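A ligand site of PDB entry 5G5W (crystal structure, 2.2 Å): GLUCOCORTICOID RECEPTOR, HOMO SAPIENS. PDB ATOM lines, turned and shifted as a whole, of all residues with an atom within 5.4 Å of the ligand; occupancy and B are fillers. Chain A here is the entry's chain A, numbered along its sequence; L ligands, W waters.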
ATOM      1  N   MET A  63      -7.524  10.051  32.841  1.00  0.00           N
ATOM      2  CA  MET A  63      -8.872  10.472  32.417  1.00  0.00           C
ATOM      3  C   MET A  63      -8.956  11.973  32.212  1.00  0.00           C
ATOM      4  O   MET A  63      -9.607  12.398  31.263  1.00  0.00           O
ATOM      5  CB  MET A  63      -9.966  10.009  33.401  1.00  0.00           C
ATOM      6  CG  MET A  63     -10.267   8.514  33.321  1.00  0.00           C
ATOM      7  SD  MET A  63     -11.956   8.063  33.921  1.00  0.00           S
ATOM      8  CE  MET A  63     -11.860   8.437  35.668  1.00  0.00           C
ATOM      9  N   LEU A  66      -6.931  12.850  29.052  1.00  0.00           N
ATOM     10  CA  LEU A  66      -7.683  12.362  27.890  1.00  0.00           C
ATOM     11  C   LEU A  66      -8.910  13.213  27.579  1.00  0.00           C
ATOM     12  O   LEU A  66      -9.242  13.366  26.417  1.00  0.00           O
ATOM     13  CB  LEU A  66      -8.042  10.871  28.043  1.00  0.00           C
ATOM     14  CG  LEU A  66      -6.840   9.902  27.911  1.00  0.00           C
ATOM     15  CD1 LEU A  66      -7.263   8.458  28.054  1.00  0.00           C
ATOM     16  CD2 LEU A  66      -6.102  10.113  26.622  1.00  0.00           C
ATOM     17  N   ASN A  67      -9.567  13.775  28.603  1.00  0.00           N
ATOM     18  CA  ASN A  67     -10.721  14.659  28.429  1.00  0.00           C
ATOM     19  C   ASN A  67     -10.242  15.950  27.809  1.00  0.00           C
ATOM     20  O   ASN A  67     -10.844  16.412  26.834  1.00  0.00           O
ATOM     21  CB  ASN A  67     -11.403  14.944  29.761  1.00  0.00           C
ATOM     22  CG  ASN A  67     -12.258  13.826  30.247  1.00  0.00           C
ATOM     23  OD1 ASN A  67     -12.527  12.887  29.521  1.00  0.00           O
ATOM     24  ND2 ASN A  67     -12.709  13.910  31.485  1.00  0.00           N
ATOM     25  N   LEU A  69      -7.458  16.398  26.035  1.00  0.00           N
ATOM     26  CA  LEU A  69      -7.070  16.020  24.666  1.00  0.00           C
ATOM     27  C   LEU A  69      -8.319  15.825  23.779  1.00  0.00           C
ATOM     28  O   LEU A  69      -8.320  16.273  22.648  1.00  0.00           O
ATOM     29  CB  LEU A  69      -6.193  14.728  24.685  1.00  0.00           C
ATOM     30  CG  LEU A  69      -5.766  14.114  23.317  1.00  0.00           C
ATOM     31  CD1 LEU A  69      -4.973  15.113  22.453  1.00  0.00           C
ATOM     32  CD2 LEU A  69      -5.018  12.791  23.533  1.00  0.00           C
ATOM     33  N   GLY A  70      -9.382  15.222  24.336  1.00  0.00           N
ATOM     34  CA  GLY A  70     -10.631  15.001  23.608  1.00  0.00           C
ATOM     35  C   GLY A  70     -11.305  16.284  23.143  1.00  0.00           C
ATOM     36  O   GLY A  70     -11.939  16.301  22.093  1.00  0.00           O
ATOM     37  N   GLN A  73      -9.474  17.268  20.085  1.00  0.00           N
ATOM     38  CA  GLN A  73      -9.843  16.354  18.997  1.00  0.00           C
ATOM     39  C   GLN A  73     -11.185  16.806  18.396  1.00  0.00           C
ATOM     40  O   GLN A  73     -11.361  16.763  17.179  1.00  0.00           O
ATOM     41  CB  GLN A  73      -9.990  14.890  19.513  1.00  0.00           C
ATOM     42  CG  GLN A  73      -8.749  14.308  20.238  1.00  0.00           C
ATOM     43  CD  GLN A  73      -7.585  13.923  19.366  1.00  0.00           C
ATOM     44  OE1 GLN A  73      -7.436  14.365  18.223  1.00  0.00           O
ATOM     45  NE2 GLN A  73      -6.721  13.061  19.870  1.00  0.00           N
ATOM     46  N   TRP A 103     -20.218  12.902  17.959  1.00  0.00           N
ATOM     47  CA  TRP A 103     -18.909  13.185  18.572  1.00  0.00           C
ATOM     48  C   TRP A 103     -18.162  11.936  19.119  1.00  0.00           C
ATOM     49  O   TRP A 103     -17.029  11.705  18.723  1.00  0.00           O
ATOM     50  CB  TRP A 103     -19.026  14.274  19.662  1.00  0.00           C
ATOM     51  CG  TRP A 103     -19.696  13.827  20.920  1.00  0.00           C
ATOM     52  CD1 TRP A 103     -21.006  13.492  21.087  1.00  0.00           C
ATOM     53  CD2 TRP A 103     -19.067  13.619  22.199  1.00  0.00           C
ATOM     54  NE1 TRP A 103     -21.236  13.061  22.369  1.00  0.00           N
ATOM     55  CE2 TRP A 103     -20.073  13.171  23.088  1.00  0.00           C
ATOM     56  CE3 TRP A 103     -17.755  13.781  22.680  1.00  0.00           C
ATOM     57  CZ2 TRP A 103     -19.815  12.917  24.438  1.00  0.00           C
ATOM     58  CZ3 TRP A 103     -17.513  13.538  24.026  1.00  0.00           C
ATOM     59  CH2 TRP A 103     -18.526  13.107  24.884  1.00  0.00           C
ATOM     60  N   MET A 104     -18.784  11.140  20.017  1.00  0.00           N
ATOM     61  CA  MET A 104     -18.119   9.969  20.611  1.00  0.00           C
ATOM     62  C   MET A 104     -17.950   8.833  19.593  1.00  0.00           C
ATOM     63  O   MET A 104     -16.968   8.081  19.664  1.00  0.00           O
ATOM     64  CB  MET A 104     -18.850   9.488  21.902  1.00  0.00           C
ATOM     65  CG  MET A 104     -18.131   8.357  22.639  1.00  0.00           C
ATOM     66  SD  MET A 104     -16.395   8.785  23.067  1.00  0.00           S
ATOM     67  CE  MET A 104     -16.693   9.786  24.506  1.00  0.00           C
ATOM     68  N   LEU A 106     -17.328   9.282  16.329  1.00  0.00           N
ATOM     69  CA  LEU A 106     -16.179   9.753  15.555  1.00  0.00           C
ATOM     70  C   LEU A 106     -14.864   9.493  16.312  1.00  0.00           C
ATOM     71  O   LEU A 106     -13.902   8.967  15.744  1.00  0.00           O
ATOM     72  CB  LEU A 106     -16.319  11.259  15.242  1.00  0.00           C
ATOM     73  CG  LEU A 106     -17.493  11.690  14.333  1.00  0.00           C
ATOM     74  CD1 LEU A 106     -17.555  13.194  14.203  1.00  0.00           C
ATOM     75  CD2 LEU A 106     -17.405  11.032  12.947  1.00  0.00           C
ATOM     76  N   MET A 107     -14.834   9.836  17.606  1.00  0.00           N
ATOM     77  CA  MET A 107     -13.649   9.673  18.420  1.00  0.00           C
ATOM     78  C   MET A 107     -13.290   8.226  18.688  1.00  0.00           C
ATOM     79  O   MET A 107     -12.122   7.854  18.528  1.00  0.00           O
ATOM     80  CB  MET A 107     -13.791  10.488  19.709  1.00  0.00           C
ATOM     81  CG  MET A 107     -13.685  11.989  19.387  1.00  0.00           C
ATOM     82  SD  MET A 107     -12.976  12.931  20.731  1.00  0.00           S
ATOM     83  CE  MET A 107     -14.276  12.677  21.998  1.00  0.00           C
ATOM     84  N   ALA A 108     -14.269   7.386  19.020  1.00  0.00           N
ATOM     85  CA  ALA A 108     -14.051   5.969  19.266  1.00  0.00           C
ATOM     86  C   ALA A 108     -13.534   5.297  17.981  1.00  0.00           C
ATOM     87  O   ALA A 108     -12.593   4.489  18.031  1.00  0.00           O
ATOM     88  CB  ALA A 108     -15.349   5.306  19.707  1.00  0.00           C
ATOM     89  N   ALA A 110     -12.115   6.882  15.198  1.00  0.00           N
ATOM     90  CA  ALA A 110     -10.796   7.381  14.828  1.00  0.00           C
ATOM     91  C   ALA A 110      -9.710   6.762  15.739  1.00  0.00           C
ATOM     92  O   ALA A 110      -8.650   6.349  15.240  1.00  0.00           O
ATOM     93  CB  ALA A 110     -10.763   8.922  14.855  1.00  0.00           C
ATOM     94  N   LEU A 111     -10.007   6.607  17.043  1.00  0.00           N
ATOM     95  CA  LEU A 111      -9.080   5.972  18.000  1.00  0.00           C
ATOM     96  C   LEU A 111      -8.857   4.468  17.681  1.00  0.00           C
ATOM     97  O   LEU A 111      -7.719   3.975  17.785  1.00  0.00           O
ATOM     98  CB  LEU A 111      -9.599   6.150  19.440  1.00  0.00           C
ATOM     99  CG  LEU A 111      -8.893   5.348  20.543  1.00  0.00           C
ATOM    100  CD1 LEU A 111      -7.400   5.740  20.682  1.00  0.00           C
ATOM    101  CD2 LEU A 111      -9.631   5.466  21.850  1.00  0.00           C
ATOM    102  N   ARG A 114      -6.501   4.310  14.609  1.00  0.00           N
ATOM    103  CA  ARG A 114      -5.176   4.729  15.070  1.00  0.00           C
ATOM    104  C   ARG A 114      -4.526   3.580  15.864  1.00  0.00           C
ATOM    105  O   ARG A 114      -3.366   3.271  15.631  1.00  0.00           O
ATOM    106  CB  ARG A 114      -5.326   6.020  15.918  1.00  0.00           C
ATOM    107  CG  ARG A 114      -4.053   6.664  16.468  1.00  0.00           C
ATOM    108  CD  ARG A 114      -3.465   7.780  15.618  1.00  0.00           C
ATOM    109  NE  ARG A 114      -4.383   8.876  15.239  1.00  0.00           N
ATOM    110  CZ  ARG A 114      -4.531  10.024  15.903  1.00  0.00           C
ATOM    111  NH1 ARG A 114      -3.908  10.228  17.057  1.00  0.00           N
ATOM    112  NH2 ARG A 114      -5.316  10.970  15.420  1.00  0.00           N
ATOM    113  N   CYS A 125      -3.977   3.860  21.346  1.00  0.00           N
ATOM    114  CA  CYS A 125      -3.073   4.933  20.954  1.00  0.00           C
ATOM    115  C   CYS A 125      -3.777   6.273  20.914  1.00  0.00           C
ATOM    116  O   CYS A 125      -3.985   6.853  19.844  1.00  0.00           O
ATOM    117  CB  CYS A 125      -2.381   4.607  19.625  1.00  0.00           C
ATOM    118  SG  CYS A 125      -1.528   3.011  19.646  1.00  0.00           S
ATOM    119  N   PHE A 126      -4.163   6.772  22.098  1.00  0.00           N
ATOM    120  CA  PHE A 126      -4.831   8.061  22.255  1.00  0.00           C
ATOM    121  C   PHE A 126      -3.949   9.176  21.746  1.00  0.00           C
ATOM    122  O   PHE A 126      -4.443  10.108  21.124  1.00  0.00           O
ATOM    123  CB  PHE A 126      -5.186   8.290  23.726  1.00  0.00           C
ATOM    124  CG  PHE A 126      -6.440   7.614  24.202  1.00  0.00           C
ATOM    125  CD1 PHE A 126      -7.685   8.224  24.037  1.00  0.00           C
ATOM    126  CD2 PHE A 126      -6.386   6.383  24.861  1.00  0.00           C
ATOM    127  CE1 PHE A 126      -8.851   7.626  24.535  1.00  0.00           C
ATOM    128  CE2 PHE A 126      -7.561   5.791  25.358  1.00  0.00           C
ATOM    129  CZ  PHE A 126      -8.777   6.405  25.182  1.00  0.00           C
ATOM    130  N   ALA A 127      -2.630   9.085  21.989  1.00  0.00           N
ATOM    131  CA  ALA A 127      -1.632  10.078  21.543  1.00  0.00           C
ATOM    132  C   ALA A 127      -0.253   9.403  21.552  1.00  0.00           C
ATOM    133  O   ALA A 127      -0.084   8.423  22.304  1.00  0.00           O
ATOM    134  CB  ALA A 127      -1.634  11.286  22.467  1.00  0.00           C
ATOM    135  N   GLN A 145     -14.077   1.387  30.800  1.00  0.00           N
ATOM    136  CA  GLN A 145     -14.300   2.374  29.753  1.00  0.00           C
ATOM    137  C   GLN A 145     -13.472   2.044  28.495  1.00  0.00           C
ATOM    138  O   GLN A 145     -14.008   2.088  27.391  1.00  0.00           O
ATOM    139  CB  GLN A 145     -14.035   3.799  30.275  1.00  0.00           C
ATOM    140  CG  GLN A 145     -14.552   4.913  29.366  1.00  0.00           C
ATOM    141  CD  GLN A 145     -16.049   5.045  29.245  1.00  0.00           C
ATOM    142  OE1 GLN A 145     -16.819   4.071  29.262  1.00  0.00           O
ATOM    143  NE2 GLN A 145     -16.499   6.273  29.024  1.00  0.00           N
ATOM    144  N   CYS A 146     -12.201   1.650  28.689  1.00  0.00           N
ATOM    145  CA  CYS A 146     -11.265   1.316  27.636  1.00  0.00           C
ATOM    146  C   CYS A 146     -11.644   0.096  26.821  1.00  0.00           C
ATOM    147  O   CYS A 146     -11.245   0.013  25.663  1.00  0.00           O
ATOM    148  CB  CYS A 146      -9.857   1.187  28.200  1.00  0.00           C
ATOM    149  SG  CYS A 146      -9.105   2.775  28.642  1.00  0.00           S
ATOM    150  N   MET A 149     -13.529   0.832  23.589  1.00  0.00           N
ATOM    151  CA  MET A 149     -12.594   1.368  22.611  1.00  0.00           C
ATOM    152  C   MET A 149     -11.802   0.195  22.003  1.00  0.00           C
ATOM    153  O   MET A 149     -11.586   0.180  20.785  1.00  0.00           O
ATOM    154  CB  MET A 149     -11.631   2.371  23.283  1.00  0.00           C
ATOM    155  CG  MET A 149     -12.296   3.665  23.786  1.00  0.00           C
ATOM    156  SD  MET A 149     -13.158   4.455  22.433  1.00  0.00           S
ATOM    157  CE  MET A 149     -13.515   6.118  23.168  1.00  0.00           C
ATOM    158  N   LEU A 235     -20.084   3.940  26.294  1.00  0.00           N
ATOM    159  CA  LEU A 235     -19.105   4.991  26.565  1.00  0.00           C
ATOM    160  C   LEU A 235     -19.767   6.190  27.240  1.00  0.00           C
ATOM    161  O   LEU A 235     -19.259   6.689  28.248  1.00  0.00           O
ATOM    162  CB  LEU A 235     -18.397   5.434  25.276  1.00  0.00           C
ATOM    163  CG  LEU A 235     -17.334   4.442  24.721  1.00  0.00           C
ATOM    164  CD1 LEU A 235     -17.023   4.752  23.279  1.00  0.00           C
ATOM    165  CD2 LEU A 235     -16.064   4.455  25.563  1.00  0.00           C
ATOM    166  N   TYR A 238     -20.993   5.932  31.132  1.00  0.00           N
ATOM    167  CA  TYR A 238     -19.909   6.223  32.062  1.00  0.00           C
ATOM    168  C   TYR A 238     -19.488   7.697  31.960  1.00  0.00           C
ATOM    169  O   TYR A 238     -19.248   8.345  32.978  1.00  0.00           O
ATOM    170  CB  TYR A 238     -18.727   5.311  31.729  1.00  0.00           C
ATOM    171  CG  TYR A 238     -17.543   5.448  32.652  1.00  0.00           C
ATOM    172  CD1 TYR A 238     -16.574   6.431  32.436  1.00  0.00           C
ATOM    173  CD2 TYR A 238     -17.337   4.554  33.698  1.00  0.00           C
ATOM    174  CE1 TYR A 238     -15.466   6.544  33.257  1.00  0.00           C
ATOM    175  CE2 TYR A 238     -16.211   4.635  34.517  1.00  0.00           C
ATOM    176  CZ  TYR A 238     -15.276   5.638  34.293  1.00  0.00           C
ATOM    177  OH  TYR A 238     -14.165   5.748  35.092  1.00  0.00           O
ATOM    178  N   CYS A 239     -19.373   8.210  30.725  1.00  0.00           N
ATOM    179  CA  CYS A 239     -18.978   9.591  30.487  1.00  0.00           C
ATOM    180  C   CYS A 239     -19.965  10.609  31.088  1.00  0.00           C
ATOM    181  O   CYS A 239     -19.514  11.571  31.734  1.00  0.00           O
ATOM    182  CB  CYS A 239     -18.742   9.839  28.999  1.00  0.00           C
ATOM    183  SG  CYS A 239     -18.200  11.510  28.634  1.00  0.00           S
ATOM    184  N   THR A 242     -19.716  10.552  35.057  1.00  0.00           N
ATOM    185  CA  THR A 242     -18.458  11.194  35.446  1.00  0.00           C
ATOM    186  C   THR A 242     -18.577  12.728  35.337  1.00  0.00           C
ATOM    187  O   THR A 242     -18.102  13.452  36.232  1.00  0.00           O
ATOM    188  CB  THR A 242     -17.312  10.608  34.609  1.00  0.00           C
ATOM    189  OG1 THR A 242     -17.296   9.201  34.837  1.00  0.00           O
ATOM    190  CG2 THR A 242     -15.972  11.150  34.999  1.00  0.00           C
ATOM    191  N   ILE A 250     -13.493  15.246  38.049  1.00  0.00           N
ATOM    192  CA  ILE A 250     -13.010  14.919  36.707  1.00  0.00           C
ATOM    193  C   ILE A 250     -13.434  16.077  35.812  1.00  0.00           C
ATOM    194  O   ILE A 250     -14.619  16.298  35.568  1.00  0.00           O
ATOM    195  CB  ILE A 250     -13.481  13.523  36.183  1.00  0.00           C
ATOM    196  CG1 ILE A 250     -12.936  12.337  37.038  1.00  0.00           C
ATOM    197  CG2 ILE A 250     -13.158  13.354  34.695  1.00  0.00           C
ATOM    198  CD1 ILE A 250     -11.470  11.921  36.844  1.00  0.00           C
ATOM    199  N   PHE A 252     -13.719  18.400  32.376  1.00  0.00           N
ATOM    200  CA  PHE A 252     -13.969  18.321  30.956  1.00  0.00           C
ATOM    201  C   PHE A 252     -13.747  19.723  30.416  1.00  0.00           C
ATOM    202  O   PHE A 252     -14.181  20.696  31.055  1.00  0.00           O
ATOM    203  CB  PHE A 252     -15.401  17.871  30.646  1.00  0.00           C
ATOM    204  CG  PHE A 252     -15.677  16.419  30.963  1.00  0.00           C
ATOM    205  CD1 PHE A 252     -15.885  15.998  32.278  1.00  0.00           C
ATOM    206  CD2 PHE A 252     -15.736  15.477  29.949  1.00  0.00           C
ATOM    207  CE1 PHE A 252     -16.130  14.667  32.564  1.00  0.00           C
ATOM    208  CE2 PHE A 252     -16.022  14.139  30.240  1.00  0.00           C
ATOM    209  CZ  PHE A 252     -16.220  13.752  31.547  1.00  0.00           C
ATOM    210  N   LEU A 256     -16.068  19.713  25.291  1.00  0.00           N
ATOM    211  CA  LEU A 256     -16.798  18.501  25.697  1.00  0.00           C
ATOM    212  C   LEU A 256     -17.932  18.806  26.656  1.00  0.00           C
ATOM    213  O   LEU A 256     -18.993  18.217  26.489  1.00  0.00           O
ATOM    214  CB  LEU A 256     -15.874  17.378  26.257  1.00  0.00           C
ATOM    215  CG  LEU A 256     -14.695  16.944  25.344  1.00  0.00           C
ATOM    216  CD1 LEU A 256     -13.983  15.730  25.932  1.00  0.00           C
ATOM    217  CD2 LEU A 256     -15.202  16.594  23.893  1.00  0.00           C
HETATM  218  C1  LIG L   1     -14.776  12.176  26.940  1.00  0.00           C
HETATM  219  C2  LIG L   1     -14.281  10.799  27.379  1.00  0.00           C
HETATM  220  C3  LIG L   1     -12.938  10.438  26.735  1.00  0.00           C
HETATM  221  C4  LIG L   1     -12.386   9.106  27.196  1.00  0.00           C
HETATM  222  C5  LIG L   1     -12.858   7.903  26.650  1.00  0.00           C
HETATM  223  C6  LIG L   1     -12.368   6.681  27.098  1.00  0.00           C
HETATM  224  C7  LIG L   1     -11.374   6.648  28.066  1.00  0.00           C
HETATM  225  C8  LIG L   1     -10.875   7.850  28.589  1.00  0.00           C
HETATM  226  C9  LIG L   1     -11.396   9.071  28.174  1.00  0.00           C
HETATM  227  O1  LIG L   1     -13.119  10.374  25.311  1.00  0.00           O
HETATM  228  C10 LIG L   1     -12.077  10.392  24.455  1.00  0.00           C
HETATM  229  C11 LIG L   1     -12.184   9.633  23.278  1.00  0.00           C
HETATM  230  C12 LIG L   1     -11.208   9.683  22.318  1.00  0.00           C
HETATM  231  C13 LIG L   1     -10.103  10.518  22.507  1.00  0.00           C
HETATM  232  C14 LIG L   1      -9.979  11.287  23.693  1.00  0.00           C
HETATM  233  C15 LIG L   1     -10.992  11.239  24.662  1.00  0.00           C
HETATM  234  C16 LIG L   1      -8.720  12.002  23.595  1.00  0.00           C
HETATM  235  N1  LIG L   1      -8.160  11.698  22.456  1.00  0.00           N
HETATM  236  N2  LIG L   1      -8.955  10.777  21.771  1.00  0.00           N
HETATM  237  C17 LIG L   1      -8.642  10.283  20.495  1.00  0.00           C
HETATM  238  C18 LIG L   1      -7.340   9.846  20.234  1.00  0.00           C
HETATM  239  C19 LIG L   1      -6.979   9.413  18.961  1.00  0.00           C
HETATM  240  C20 LIG L   1      -7.946   9.438  17.955  1.00  0.00           C
HETATM  241  C21 LIG L   1      -9.246   9.894  18.200  1.00  0.00           C
HETATM  242  C22 LIG L   1      -9.603  10.330  19.465  1.00  0.00           C
HETATM  243  F1  LIG L   1      -7.624   9.015  16.726  1.00  0.00           F
HETATM  244  N3  LIG L   1     -14.143  10.759  28.834  1.00  0.00           N
HETATM  245  C23 LIG L   1     -14.736   9.801  29.585  1.00  0.00           C
HETATM  246  O2  LIG L   1     -15.434   8.913  29.090  1.00  0.00           O
HETATM  247  C24 LIG L   1     -14.499   9.804  31.078  1.00  0.00           C
HETATM  248  F2  LIG L   1     -15.704   9.762  31.745  1.00  0.00           F
HETATM  249  F3  LIG L   1     -13.768   8.664  31.385  1.00  0.00           F
HETATM  250  F4  LIG L   1     -13.794  10.895  31.546  1.00  0.00           F
HETATM  251  O   HOH W   1     -11.151  11.958  16.551  1.00  0.00           O
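OD1 of Asn 67 sits close to O of Met 63, at 3.4 Å. The side-chain amide nitrogen (NE2) of Gln 145 sits at hydrogen-bond distance from the backbone carbonyl oxygen (O) of Leu 235 (2.9 Å). SD of Met 63 lies within hydrogen-bond range of OH of Tyr 238, at 3.4 Å. The backbone carbonyl oxygen of Tyr 238 is in hydrogen-bond range of the side-chain hydroxyl of Thr 242 (2.8 Å).
OD1 of Asn 67 lies within hydrogen-bond range of N3 of the ligand (2.8 Å). The side-chain amide nitrogen (NE2) of Gln 145 sits at hydrogen-bond distance from an oxygen (O2) of the ligand (2.8 Å). The side-chain amide nitrogen of Gln 73 sits at hydrogen-bond distance from a nitrogen (N1) of the ligand.
The side-chain sulfur of Met 63 sits close to a fluorine (F3) of the ligand (3.2 Å). The backbone carbonyl oxygen (O) of Ala 110 lies close to a fluorine (F1) of the ligand. N of Leu 111 sits close to F1 of the ligand (3.4 Å). NH2 of Arg 114 lies close to F1 of the ligand, 3.3 Å away. Merely in contact with the ligand: Phe 126, Leu 66, Tyr 238, Gly 70, Thr 242, Cys 239, Leu 69, Met 107, Met 104, Phe 252, Met 149 and Leu 256. Hydrophobic or aromatic side chains within 4 Å of the ligand: Met 63, Leu 66, Leu 69, Met 104, Met 107, Ala 110, Leu 111, Phe 126, Met 149, Tyr 238, Phe 252 and Leu 256. Within 4 Å of the ligand: Met 63, Leu 66, Asn 67, Leu 69, Gly 70, Gln 73, Met 104, Met 107, Ala 110, Leu 111, Arg 114, Phe 126, Gln 145, Met 149, Tyr 238, Cys 239, Thr 242, Phe 252 and Leu 256.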
